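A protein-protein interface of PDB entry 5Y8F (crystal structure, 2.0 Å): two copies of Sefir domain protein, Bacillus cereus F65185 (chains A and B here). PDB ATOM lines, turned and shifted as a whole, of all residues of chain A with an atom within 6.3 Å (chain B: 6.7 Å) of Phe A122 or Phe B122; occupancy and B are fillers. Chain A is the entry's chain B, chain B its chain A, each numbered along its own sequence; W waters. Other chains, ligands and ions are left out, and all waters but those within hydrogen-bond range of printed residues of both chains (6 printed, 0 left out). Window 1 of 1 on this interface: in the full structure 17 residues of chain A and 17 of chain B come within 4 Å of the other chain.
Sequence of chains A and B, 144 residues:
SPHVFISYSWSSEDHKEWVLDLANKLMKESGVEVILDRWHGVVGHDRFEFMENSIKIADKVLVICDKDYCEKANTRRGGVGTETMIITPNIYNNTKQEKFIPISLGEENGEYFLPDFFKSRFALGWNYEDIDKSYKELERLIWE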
ATOM      1  N   PHE A 100      27.910   4.489 -32.501  1.00  0.00           N
ATOM      2  CA  PHE A 100      28.615   3.594 -31.593  1.00  0.00           C
ATOM      3  C   PHE A 100      27.683   2.556 -30.983  1.00  0.00           C
ATOM      4  O   PHE A 100      26.625   2.889 -30.437  1.00  0.00           O
ATOM      5  CB  PHE A 100      29.300   4.403 -30.496  1.00  0.00           C
ATOM      6  CG  PHE A 100      30.335   5.354 -31.016  1.00  0.00           C
ATOM      7  CD1 PHE A 100      31.477   4.877 -31.641  1.00  0.00           C
ATOM      8  CD2 PHE A 100      30.168   6.721 -30.889  1.00  0.00           C
ATOM      9  CE1 PHE A 100      32.433   5.748 -32.127  1.00  0.00           C
ATOM     10  CE2 PHE A 100      31.122   7.596 -31.374  1.00  0.00           C
ATOM     11  CZ  PHE A 100      32.255   7.109 -31.992  1.00  0.00           C
ATOM     12  N   ILE A 101      28.095   1.294 -31.068  1.00  0.00           N
ATOM     13  CA  ILE A 101      27.418   0.180 -30.410  1.00  0.00           C
ATOM     14  C   ILE A 101      28.429  -0.508 -29.501  1.00  0.00           C
ATOM     15  O   ILE A 101      29.125  -1.441 -29.931  1.00  0.00           O
ATOM     16  CB  ILE A 101      26.817  -0.799 -31.432  1.00  0.00           C
ATOM     17  CG1 ILE A 101      25.900  -0.057 -32.409  1.00  0.00           C
ATOM     18  CG2 ILE A 101      26.055  -1.913 -30.732  1.00  0.00           C
ATOM     19  CD1 ILE A 101      25.308  -0.947 -33.485  1.00  0.00           C
ATOM     20  N   PRO A 102      28.584  -0.060 -28.259  1.00  0.00           N
ATOM     21  CA  PRO A 102      29.540  -0.720 -27.365  1.00  0.00           C
ATOM     22  C   PRO A 102      29.042  -2.098 -26.968  1.00  0.00           C
ATOM     23  O   PRO A 102      27.868  -2.284 -26.641  1.00  0.00           O
ATOM     24  CB  PRO A 102      29.605   0.220 -26.157  1.00  0.00           C
ATOM     25  CG  PRO A 102      29.087   1.535 -26.663  1.00  0.00           C
ATOM     26  CD  PRO A 102      28.042   1.174 -27.669  1.00  0.00           C
ATOM     27  N   ILE A 103      29.946  -3.071 -27.018  1.00  0.00           N
ATOM     28  CA  ILE A 103      29.666  -4.440 -26.602  1.00  0.00           C
ATOM     29  C   ILE A 103      30.610  -4.772 -25.458  1.00  0.00           C
ATOM     30  O   ILE A 103      31.834  -4.786 -25.642  1.00  0.00           O
ATOM     31  CB  ILE A 103      29.830  -5.442 -27.754  1.00  0.00           C
ATOM     32  CG1 ILE A 103      28.978  -5.024 -28.954  1.00  0.00           C
ATOM     33  CG2 ILE A 103      29.439  -6.837 -27.298  1.00  0.00           C
ATOM     34  CD1 ILE A 103      29.139  -5.933 -30.151  1.00  0.00           C
ATOM     35  N   LEU A 114      33.017  -0.095 -20.393  1.00  0.00           N
ATOM     36  CA  LEU A 114      32.790   1.045 -21.269  1.00  0.00           C
ATOM     37  C   LEU A 114      33.756   2.171 -20.921  1.00  0.00           C
ATOM     38  O   LEU A 114      33.826   2.585 -19.757  1.00  0.00           O
ATOM     39  CB  LEU A 114      31.341   1.525 -21.158  1.00  0.00           C
ATOM     40  CG  LEU A 114      30.900   2.586 -22.159  1.00  0.00           C
ATOM     41  CD1 LEU A 114      31.009   2.048 -23.565  1.00  0.00           C
ATOM     42  CD2 LEU A 114      29.474   3.000 -21.871  1.00  0.00           C
ATOM     43  N   PHE A 118      32.684   7.890 -22.846  1.00  0.00           N
ATOM     44  CA  PHE A 118      31.392   7.668 -23.490  1.00  0.00           C
ATOM     45  C   PHE A 118      30.302   8.337 -22.664  1.00  0.00           C
ATOM     46  O   PHE A 118      30.065   7.960 -21.512  1.00  0.00           O
ATOM     47  CB  PHE A 118      31.123   6.176 -23.657  1.00  0.00           C
ATOM     48  CG  PHE A 118      31.781   5.580 -24.865  1.00  0.00           C
ATOM     49  CD1 PHE A 118      33.133   5.288 -24.857  1.00  0.00           C
ATOM     50  CD2 PHE A 118      31.050   5.319 -26.011  1.00  0.00           C
ATOM     51  CE1 PHE A 118      33.746   4.743 -25.972  1.00  0.00           C
ATOM     52  CE2 PHE A 118      31.655   4.771 -27.127  1.00  0.00           C
ATOM     53  CZ  PHE A 118      33.004   4.484 -27.107  1.00  0.00           C
ATOM     54  N   SER A 120      26.955   8.562 -23.204  1.00  0.00           N
ATOM     55  CA  SER A 120      25.882   7.601 -22.981  1.00  0.00           C
ATOM     56  C   SER A 120      26.475   6.302 -22.457  1.00  0.00           C
ATOM     57  O   SER A 120      27.468   5.804 -22.997  1.00  0.00           O
ATOM     58  CB  SER A 120      25.103   7.344 -24.266  1.00  0.00           C
ATOM     59  OG  SER A 120      24.062   6.413 -24.030  1.00  0.00           O
ATOM     60  N   ARG A 121      25.887   5.760 -21.394  1.00  0.00           N
ATOM     61  CA  ARG A 121      26.470   4.594 -20.750  1.00  0.00           C
ATOM     62  C   ARG A 121      25.875   3.279 -21.251  1.00  0.00           C
ATOM     63  O   ARG A 121      26.122   2.231 -20.645  1.00  0.00           O
ATOM     64  CB  ARG A 121      26.339   4.707 -19.231  1.00  0.00           C
ATOM     65  CG  ARG A 121      26.905   6.026 -18.705  1.00  0.00           C
ATOM     66  CD  ARG A 121      28.390   6.210 -19.022  1.00  0.00           C
ATOM     67  NE  ARG A 121      29.240   5.123 -18.555  1.00  0.00           N
ATOM     68  CZ  ARG A 121      30.452   4.871 -19.040  1.00  0.00           C
ATOM     69  NH1 ARG A 121      30.954   5.631 -20.006  1.00  0.00           N
ATOM     70  NH2 ARG A 121      31.165   3.862 -18.556  1.00  0.00           N
ATOM     71  N   PHE A 122      25.097   3.310 -22.332  1.00  0.00           N
ATOM     72  CA  PHE A 122      24.526   2.087 -22.883  1.00  0.00           C
ATOM     73  C   PHE A 122      25.616   1.191 -23.454  1.00  0.00           C
ATOM     74  O   PHE A 122      26.594   1.666 -24.038  1.00  0.00           O
ATOM     75  CB  PHE A 122      23.519   2.400 -23.989  1.00  0.00           C
ATOM     76  CG  PHE A 122      22.125   2.680 -23.500  1.00  0.00           C
ATOM     77  CD1 PHE A 122      21.338   1.662 -22.987  1.00  0.00           C
ATOM     78  CD2 PHE A 122      21.590   3.950 -23.595  1.00  0.00           C
ATOM     79  CE1 PHE A 122      20.046   1.922 -22.551  1.00  0.00           C
ATOM     80  CE2 PHE A 122      20.305   4.212 -23.161  1.00  0.00           C
ATOM     81  CZ  PHE A 122      19.536   3.197 -22.641  1.00  0.00           C
ATOM     82  N   ALA A 123      25.428  -0.115 -23.294  1.00  0.00           N
ATOM     83  CA  ALA A 123      26.318  -1.107 -23.873  1.00  0.00           C
ATOM     84  C   ALA A 123      25.558  -2.418 -23.977  1.00  0.00           C
ATOM     85  O   ALA A 123      24.691  -2.712 -23.150  1.00  0.00           O
ATOM     86  CB  ALA A 123      27.592  -1.294 -23.042  1.00  0.00           C
ATOM     87  N   LEU A 124      25.874  -3.185 -25.017  1.00  0.00           N
ATOM     88  CA  LEU A 124      25.324  -4.528 -25.167  1.00  0.00           C
ATOM     89  C   LEU A 124      26.122  -5.474 -24.278  1.00  0.00           C
ATOM     90  O   LEU A 124      27.285  -5.777 -24.566  1.00  0.00           O
ATOM     91  CB  LEU A 124      25.368  -4.973 -26.626  1.00  0.00           C
ATOM     92  CG  LEU A 124      25.012  -6.438 -26.893  1.00  0.00           C
ATOM     93  CD1 LEU A 124      23.646  -6.781 -26.312  1.00  0.00           C
ATOM     94  CD2 LEU A 124      25.054  -6.739 -28.385  1.00  0.00           C
ATOM     95  N   GLU A 137      20.113  -8.974 -30.388  1.00  0.00           N
ATOM     96  CA  GLU A 137      20.064  -7.567 -30.010  1.00  0.00           C
ATOM     97  C   GLU A 137      21.094  -6.765 -30.790  1.00  0.00           C
ATOM     98  O   GLU A 137      20.822  -5.624 -31.192  1.00  0.00           O
ATOM     99  CB  GLU A 137      20.279  -7.434 -28.504  1.00  0.00           C
ATOM    100  CG  GLU A 137      20.497  -6.010 -28.034  1.00  0.00           C
ATOM    101  CD  GLU A 137      19.255  -5.133 -28.166  1.00  0.00           C
ATOM    102  OE1 GLU A 137      18.193  -5.617 -28.617  1.00  0.00           O
ATOM    103  OE2 GLU A 137      19.339  -3.944 -27.795  1.00  0.00           O
ATOM    104  N   ARG A 140      19.591  -5.902 -34.013  1.00  0.00           N
ATOM    105  CA  ARG A 140      18.632  -4.810 -33.876  1.00  0.00           C
ATOM    106  C   ARG A 140      19.345  -3.471 -33.742  1.00  0.00           C
ATOM    107  O   ARG A 140      18.934  -2.479 -34.354  1.00  0.00           O
ATOM    108  CB  ARG A 140      17.721  -5.052 -32.672  1.00  0.00           C
ATOM    109  CG  ARG A 140      16.567  -4.061 -32.565  1.00  0.00           C
ATOM    110  CD  ARG A 140      15.865  -4.148 -31.216  1.00  0.00           C
ATOM    111  NE  ARG A 140      16.740  -3.747 -30.116  1.00  0.00           N
ATOM    112  CZ  ARG A 140      16.881  -2.495 -29.690  1.00  0.00           C
ATOM    113  NH1 ARG A 140      16.205  -1.518 -30.275  1.00  0.00           N
ATOM    114  NH2 ARG A 140      17.697  -2.219 -28.681  1.00  0.00           N
ATOM    115  N   LEU A 141      20.416  -3.425 -32.946  1.00  0.00           N
ATOM    116  CA  LEU A 141      21.165  -2.185 -32.776  1.00  0.00           C
ATOM    117  C   LEU A 141      21.816  -1.740 -34.080  1.00  0.00           C
ATOM    118  O   LEU A 141      21.996  -0.538 -34.309  1.00  0.00           O
ATOM    119  CB  LEU A 141      22.221  -2.367 -31.682  1.00  0.00           C
ATOM    120  CG  LEU A 141      21.686  -2.588 -30.261  1.00  0.00           C
ATOM    121  CD1 LEU A 141      22.778  -3.100 -29.326  1.00  0.00           C
ATOM    122  CD2 LEU A 141      21.067  -1.312 -29.711  1.00  0.00           C
ATOM    123  N   GLU B  98      23.127  11.841 -25.488  1.00  0.00           N
ATOM    124  CA  GLU B  98      23.399  11.053 -24.291  1.00  0.00           C
ATOM    125  C   GLU B  98      22.355  11.261 -23.204  1.00  0.00           C
ATOM    126  O   GLU B  98      22.323  10.483 -22.244  1.00  0.00           O
ATOM    127  CB  GLU B  98      24.787  11.389 -23.736  1.00  0.00           C
ATOM    128  CG  GLU B  98      24.916  12.797 -23.161  1.00  0.00           C
ATOM    129  CD  GLU B  98      25.387  13.811 -24.184  1.00  0.00           C
ATOM    130  OE1 GLU B  98      25.269  13.537 -25.397  1.00  0.00           O
ATOM    131  OE2 GLU B  98      25.886  14.879 -23.771  1.00  0.00           O
ATOM    132  N   PHE B 100      19.137  10.848 -23.488  1.00  0.00           N
ATOM    133  CA  PHE B 100      18.019   9.925 -23.613  1.00  0.00           C
ATOM    134  C   PHE B 100      18.355   8.558 -23.031  1.00  0.00           C
ATOM    135  O   PHE B 100      19.384   7.962 -23.361  1.00  0.00           O
ATOM    136  CB  PHE B 100      17.615   9.793 -25.081  1.00  0.00           C
ATOM    137  CG  PHE B 100      17.123  11.078 -25.689  1.00  0.00           C
ATOM    138  CD1 PHE B 100      15.951  11.667 -25.239  1.00  0.00           C
ATOM    139  CD2 PHE B 100      17.832  11.700 -26.702  1.00  0.00           C
ATOM    140  CE1 PHE B 100      15.492  12.850 -25.794  1.00  0.00           C
ATOM    141  CE2 PHE B 100      17.380  12.887 -27.260  1.00  0.00           C
ATOM    142  CZ  PHE B 100      16.208  13.460 -26.806  1.00  0.00           C
ATOM    143  N   ILE B 101      17.479   8.075 -22.153  1.00  0.00           N
ATOM    144  CA  ILE B 101      17.525   6.719 -21.613  1.00  0.00           C
ATOM    145  C   ILE B 101      16.185   6.060 -21.904  1.00  0.00           C
ATOM    146  O   ILE B 101      15.266   6.140 -21.076  1.00  0.00           O
ATOM    147  CB  ILE B 101      17.817   6.709 -20.102  1.00  0.00           C
ATOM    148  CG1 ILE B 101      19.091   7.489 -19.784  1.00  0.00           C
ATOM    149  CG2 ILE B 101      17.915   5.278 -19.591  1.00  0.00           C
ATOM    150  CD1 ILE B 101      19.396   7.545 -18.288  1.00  0.00           C
ATOM    151  N   PRO B 102      16.006   5.442 -23.069  1.00  0.00           N
ATOM    152  CA  PRO B 102      14.724   4.794 -23.363  1.00  0.00           C
ATOM    153  C   PRO B 102      14.537   3.531 -22.535  1.00  0.00           C
ATOM    154  O   PRO B 102      15.457   2.724 -22.381  1.00  0.00           O
ATOM    155  CB  PRO B 102      14.824   4.472 -24.857  1.00  0.00           C
ATOM    156  CG  PRO B 102      15.911   5.364 -25.380  1.00  0.00           C
ATOM    157  CD  PRO B 102      16.888   5.467 -24.247  1.00  0.00           C
ATOM    158  N   ILE B 103      13.329   3.368 -22.003  1.00  0.00           N
ATOM    159  CA  ILE B 103      12.948   2.186 -21.235  1.00  0.00           C
ATOM    160  C   ILE B 103      11.807   1.513 -21.986  1.00  0.00           C
ATOM    161  O   ILE B 103      10.708   2.075 -22.090  1.00  0.00           O
ATOM    162  CB  ILE B 103      12.521   2.533 -19.802  1.00  0.00           C
ATOM    163  CG1 ILE B 103      13.599   3.343 -19.083  1.00  0.00           C
ATOM    164  CG2 ILE B 103      12.219   1.267 -19.014  1.00  0.00           C
ATOM    165  CD1 ILE B 103      13.183   3.772 -17.686  1.00  0.00           C
ATOM    166  N   LEU B 114      10.630   1.139 -29.265  1.00  0.00           N
ATOM    167  CA  LEU B 114      11.441   2.337 -29.418  1.00  0.00           C
ATOM    168  C   LEU B 114      11.002   3.066 -30.682  1.00  0.00           C
ATOM    169  O   LEU B 114      10.956   2.452 -31.754  1.00  0.00           O
ATOM    170  CB  LEU B 114      12.928   1.980 -29.488  1.00  0.00           C
ATOM    171  CG  LEU B 114      13.896   3.159 -29.436  1.00  0.00           C
ATOM    172  CD1 LEU B 114      13.749   3.874 -28.112  1.00  0.00           C
ATOM    173  CD2 LEU B 114      15.325   2.695 -29.636  1.00  0.00           C
ATOM    174  N   PHE B 118      14.418   7.352 -33.354  1.00  0.00           N
ATOM    175  CA  PHE B 118      15.555   7.356 -32.439  1.00  0.00           C
ATOM    176  C   PHE B 118      16.743   6.738 -33.171  1.00  0.00           C
ATOM    177  O   PHE B 118      16.753   5.532 -33.442  1.00  0.00           O
ATOM    178  CB  PHE B 118      15.222   6.580 -31.165  1.00  0.00           C
ATOM    179  CG  PHE B 118      14.417   7.363 -30.153  1.00  0.00           C
ATOM    180  CD1 PHE B 118      13.404   8.221 -30.556  1.00  0.00           C
ATOM    181  CD2 PHE B 118      14.674   7.233 -28.795  1.00  0.00           C
ATOM    182  CE1 PHE B 118      12.660   8.936 -29.624  1.00  0.00           C
ATOM    183  CE2 PHE B 118      13.936   7.943 -27.859  1.00  0.00           C
ATOM    184  CZ  PHE B 118      12.930   8.797 -28.274  1.00  0.00           C
ATOM    185  N   LYS B 119      17.744   7.561 -33.500  1.00  0.00           N
ATOM    186  CA  LYS B 119      18.852   7.086 -34.328  1.00  0.00           C
ATOM    187  C   LYS B 119      19.672   6.023 -33.608  1.00  0.00           C
ATOM    188  O   LYS B 119      20.100   5.040 -34.224  1.00  0.00           O
ATOM    189  CB  LYS B 119      19.740   8.250 -34.755  1.00  0.00           C
ATOM    190  CG  LYS B 119      19.030   9.302 -35.589  1.00  0.00           C
ATOM    191  CD  LYS B 119      20.042  10.246 -36.210  1.00  0.00           C
ATOM    192  CE  LYS B 119      19.476  11.634 -36.371  1.00  0.00           C
ATOM    193  NZ  LYS B 119      19.664  12.416 -35.110  1.00  0.00           N
ATOM    194  N   SER B 120      19.921   6.208 -32.316  1.00  0.00           N
ATOM    195  CA  SER B 120      20.514   5.144 -31.523  1.00  0.00           C
ATOM    196  C   SER B 120      19.412   4.196 -31.073  1.00  0.00           C
ATOM    197  O   SER B 120      18.381   4.629 -30.552  1.00  0.00           O
ATOM    198  CB  SER B 120      21.257   5.711 -30.316  1.00  0.00           C
ATOM    199  OG  SER B 120      21.844   4.664 -29.567  1.00  0.00           O
ATOM    200  N   ARG B 121      19.630   2.903 -31.272  1.00  0.00           N
ATOM    201  CA  ARG B 121      18.613   1.898 -31.002  1.00  0.00           C
ATOM    202  C   ARG B 121      18.690   1.327 -29.593  1.00  0.00           C
ATOM    203  O   ARG B 121      17.936   0.399 -29.275  1.00  0.00           O
ATOM    204  CB  ARG B 121      18.740   0.766 -32.025  1.00  0.00           C
ATOM    205  CG  ARG B 121      18.436   1.152 -33.465  1.00  0.00           C
ATOM    206  CD  ARG B 121      16.928   1.281 -33.667  1.00  0.00           C
ATOM    207  NE  ARG B 121      16.341   2.587 -33.420  1.00  0.00           N
ATOM    208  CZ  ARG B 121      15.043   2.766 -33.187  1.00  0.00           C
ATOM    209  NH1 ARG B 121      14.223   1.723 -33.162  1.00  0.00           N
ATOM    210  NH2 ARG B 121      14.566   3.980 -32.976  1.00  0.00           N
ATOM    211  N   PHE B 122      19.537   1.888 -28.732  1.00  0.00           N
ATOM    212  CA  PHE B 122      19.662   1.381 -27.372  1.00  0.00           C
ATOM    213  C   PHE B 122      18.402   1.661 -26.567  1.00  0.00           C
ATOM    214  O   PHE B 122      17.781   2.720 -26.696  1.00  0.00           O
ATOM    215  CB  PHE B 122      20.868   2.008 -26.670  1.00  0.00           C
ATOM    216  CG  PHE B 122      22.173   1.327 -26.983  1.00  0.00           C
ATOM    217  CD1 PHE B 122      22.452   0.060 -26.491  1.00  0.00           C
ATOM    218  CD2 PHE B 122      23.119   1.957 -27.769  1.00  0.00           C
ATOM    219  CE1 PHE B 122      23.652  -0.562 -26.786  1.00  0.00           C
ATOM    220  CE2 PHE B 122      24.318   1.341 -28.066  1.00  0.00           C
ATOM    221  CZ  PHE B 122      24.586   0.080 -27.575  1.00  0.00           C
ATOM    222  N   ALA B 123      18.041   0.707 -25.716  1.00  0.00           N
ATOM    223  CA  ALA B 123      16.918   0.861 -24.808  1.00  0.00           C
ATOM    224  C   ALA B 123      17.104  -0.111 -23.658  1.00  0.00           C
ATOM    225  O   ALA B 123      17.642  -1.207 -23.835  1.00  0.00           O
ATOM    226  CB  ALA B 123      15.580   0.608 -25.510  1.00  0.00           C
ATOM    227  N   LEU B 124      16.672   0.312 -22.474  1.00  0.00           N
ATOM    228  CA  LEU B 124      16.660  -0.556 -21.303  1.00  0.00           C
ATOM    229  C   LEU B 124      15.421  -1.443 -21.365  1.00  0.00           C
ATOM    230  O   LEU B 124      14.302  -0.972 -21.153  1.00  0.00           O
ATOM    231  CB  LEU B 124      16.674   0.273 -20.023  1.00  0.00           C
ATOM    232  CG  LEU B 124      16.457  -0.499 -18.719  1.00  0.00           C
ATOM    233  CD1 LEU B 124      17.466  -1.627 -18.567  1.00  0.00           C
ATOM    234  CD2 LEU B 124      16.494   0.440 -17.519  1.00  0.00           C
ATOM    235  N   GLY B 125      15.613  -2.723 -21.667  1.00  0.00           N
ATOM    236  CA  GLY B 125      14.500  -3.652 -21.649  1.00  0.00           C
ATOM    237  C   GLY B 125      14.055  -3.956 -20.233  1.00  0.00           C
ATOM    238  O   GLY B 125      14.726  -4.704 -19.518  1.00  0.00           O
ATOM    239  N   GLU B 137      20.390  -1.291 -13.491  1.00  0.00           N
ATOM    240  CA  GLU B 137      20.934  -0.782 -14.745  1.00  0.00           C
ATOM    241  C   GLU B 137      20.434   0.626 -15.043  1.00  0.00           C
ATOM    242  O   GLU B 137      21.184   1.456 -15.567  1.00  0.00           O
ATOM    243  CB  GLU B 137      20.590  -1.741 -15.885  1.00  0.00           C
ATOM    244  CG  GLU B 137      20.863  -1.214 -17.281  1.00  0.00           C
ATOM    245  CD  GLU B 137      22.340  -1.063 -17.604  1.00  0.00           C
ATOM    246  OE1 GLU B 137      23.192  -1.375 -16.746  1.00  0.00           O
ATOM    247  OE2 GLU B 137      22.647  -0.645 -18.739  1.00  0.00           O
ATOM    248  N   ARG B 140      22.541   2.936 -13.119  1.00  0.00           N
ATOM    249  CA  ARG B 140      23.847   3.096 -13.751  1.00  0.00           C
ATOM    250  C   ARG B 140      23.769   4.007 -14.969  1.00  0.00           C
ATOM    251  O   ARG B 140      24.653   4.844 -15.182  1.00  0.00           O
ATOM    252  CB  ARG B 140      24.411   1.733 -14.148  1.00  0.00           C
ATOM    253  CG  ARG B 140      25.846   1.781 -14.640  1.00  0.00           C
ATOM    254  CD  ARG B 140      26.258   0.464 -15.282  1.00  0.00           C
ATOM    255  NE  ARG B 140      25.512   0.189 -16.507  1.00  0.00           N
ATOM    256  CZ  ARG B 140      25.881   0.597 -17.718  1.00  0.00           C
ATOM    257  NH1 ARG B 140      26.994   1.301 -17.875  1.00  0.00           N
ATOM    258  NH2 ARG B 140      25.141   0.296 -18.775  1.00  0.00           N
ATOM    259  N   LEU B 141      22.725   3.850 -15.789  1.00  0.00           N
ATOM    260  CA  LEU B 141      22.586   4.692 -16.972  1.00  0.00           C
ATOM    261  C   LEU B 141      22.408   6.156 -16.591  1.00  0.00           C
ATOM    262  O   LEU B 141      22.854   7.048 -17.322  1.00  0.00           O
ATOM    263  CB  LEU B 141      21.411   4.196 -17.818  1.00  0.00           C
ATOM    264  CG  LEU B 141      21.598   2.818 -18.462  1.00  0.00           C
ATOM    265  CD1 LEU B 141      20.282   2.248 -18.967  1.00  0.00           C
ATOM    266  CD2 LEU B 141      22.608   2.891 -19.601  1.00  0.00           C
HETATM  267  O   HOH W   1      23.843   3.121 -31.344  1.00  0.00           O
HETATM  268  O   HOH W   2      23.038  -1.166 -21.656  1.00  0.00           O
HETATM  269  O   HOH W   3      19.373  -1.932 -26.075  1.00  0.00           O
HETATM  270  O   HOH W   4      23.693   6.777 -20.075  1.00  0.00           O
HETATM  271  O   HOH W   5      21.950   1.684 -32.730  1.00  0.00           O
HETATM  272  O   HOH W   6      22.105   7.786 -22.198  1.00  0.00           O
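Phe A118 touches none of the printed residues of chain B. Printed residues of chain B within 4 Å of Arg A121: Arg B140 and Leu B141. Of the printed residues of chain B, Phe A122 touches Phe B100, Pro B102, Phe B122, Ala B123, Leu B124 and Leu B141. Ile B103 touches none of the printed residues of chain A. Of the printed residues of chain A, Arg B140 touches Arg A121 (2.9 Å). The nearest printed residue of chain A that does not touch Phe B122 is Ile A101 (4.01 Å). The nearest printed residue of chain A that does not touch Glu B98 is Arg A121 (6.0 Å).
O of Arg B121 lies within hydrogen-bond range of NH2 of Arg A140, at 2.7 Å. The guanidinium group (NH2) of Arg B140 is in hydrogen-bond range of the backbone carbonyl oxygen (O) of Arg A121, at 2.9 Å.
O of Phe A100 touches CE2 of Phe B122, at 3.7 Å. Pro A102 touches Phe B122 (CD to CZ, 3.6 Å). Glu B98 touches Ser A120 (CB to N, 3.6 Å). Arg A121 touches Leu B141. Phe A122 touches Phe B100. Ala B123 touches Phe A122 (C to CE1, 3.7 Å). Phe A122 touches Leu B124 (CE1 to N, 3.7 Å). CD1 of Leu B141 touches CE1 of Phe A122, at 3.6 Å. Ala A123 touches Phe B122. CD2 of Leu A141 touches C of Arg B121, at 3.6 Å.
Phe A100 touches Phe B122, and with the chains exchanged Phe A122 touches Phe B100. Arg A121 touches Arg B140, and with the chains exchanged Arg A140 touches Arg B121. Arg A121 touches Leu B141, and with the chains exchanged Leu A141 touches Arg B121. Phe A122 touches Leu B124, and with the chains exchanged Leu A124 touches Phe B122.
The backbone carbonyl oxygen of Pro A102 is in hydrogen-bond range of the backbone NH of Leu A124, at 2.7 Å. NH2 of Arg A140 is in salt-bridge range of OE2 of Glu A137 (2.5 Å). The side-chain carboxylate (OE2) of Glu B137 lies within salt-bridge range of the guanidinium group (NH2) of Arg B140. The backbone carbonyl oxygen (O) of Pro B102 lies within hydrogen-bond range of the backbone NH (N) of Leu B124 (2.7 Å). The backbone carbonyl oxygen of Phe A118 is in hydrogen-bond range of the guanidinium group of Arg A121, at 2.9 Å. The backbone carbonyl oxygen (O) of Leu A114 sits at hydrogen-bond distance from the guanidinium group (NH2) of Arg A121 (3.2 Å).
Water W3 lies within hydrogen-bond range of OE2 of Glu A137, O of Ala B123 and NH2 of Arg A140. Water W6 lies within hydrogen-bond range of the backbone carbonyl oxygen (O) of Glu B98 (2.7 Å), the backbone carbonyl oxygen (O) of Phe B100 (3.0 Å) and the side-chain hydroxyl (OG) of Ser A120 (3.0 Å). Water W2 bridges O of Ala A123 (2.7 Å) and OE2 of Glu B137 (3.0 Å). Water W5 bridges O of Leu A141 and N of Arg B121. Water W4 lies within hydrogen-bond range of the backbone NH of Arg A121 and the backbone carbonyl oxygen of Leu B141. Water W1 lies within hydrogen-bond range of the backbone carbonyl oxygen of Phe A100 (2.9 Å) and the side-chain hydroxyl of Ser B120 (3.1 Å).
Hydrophobic or aromatic side chains of chain A within 4 Å of the printed part of chain B: Pro A102, Phe A122 and Leu A141. Of the 17 printed residues of chain B, 9 touch a printed residue of chain A. Printed residues of chain B that touch a printed residue of chain A: Glu B98, Phe B100, Pro B102, Arg B121, Phe B122, Ala B123, Leu B124, Arg B140 and Leu B141. Among the printed residues, no Asp or Glu carboxylate lies within 4 Å of a Lys or Arg side-chain nitrogen of the other chain.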
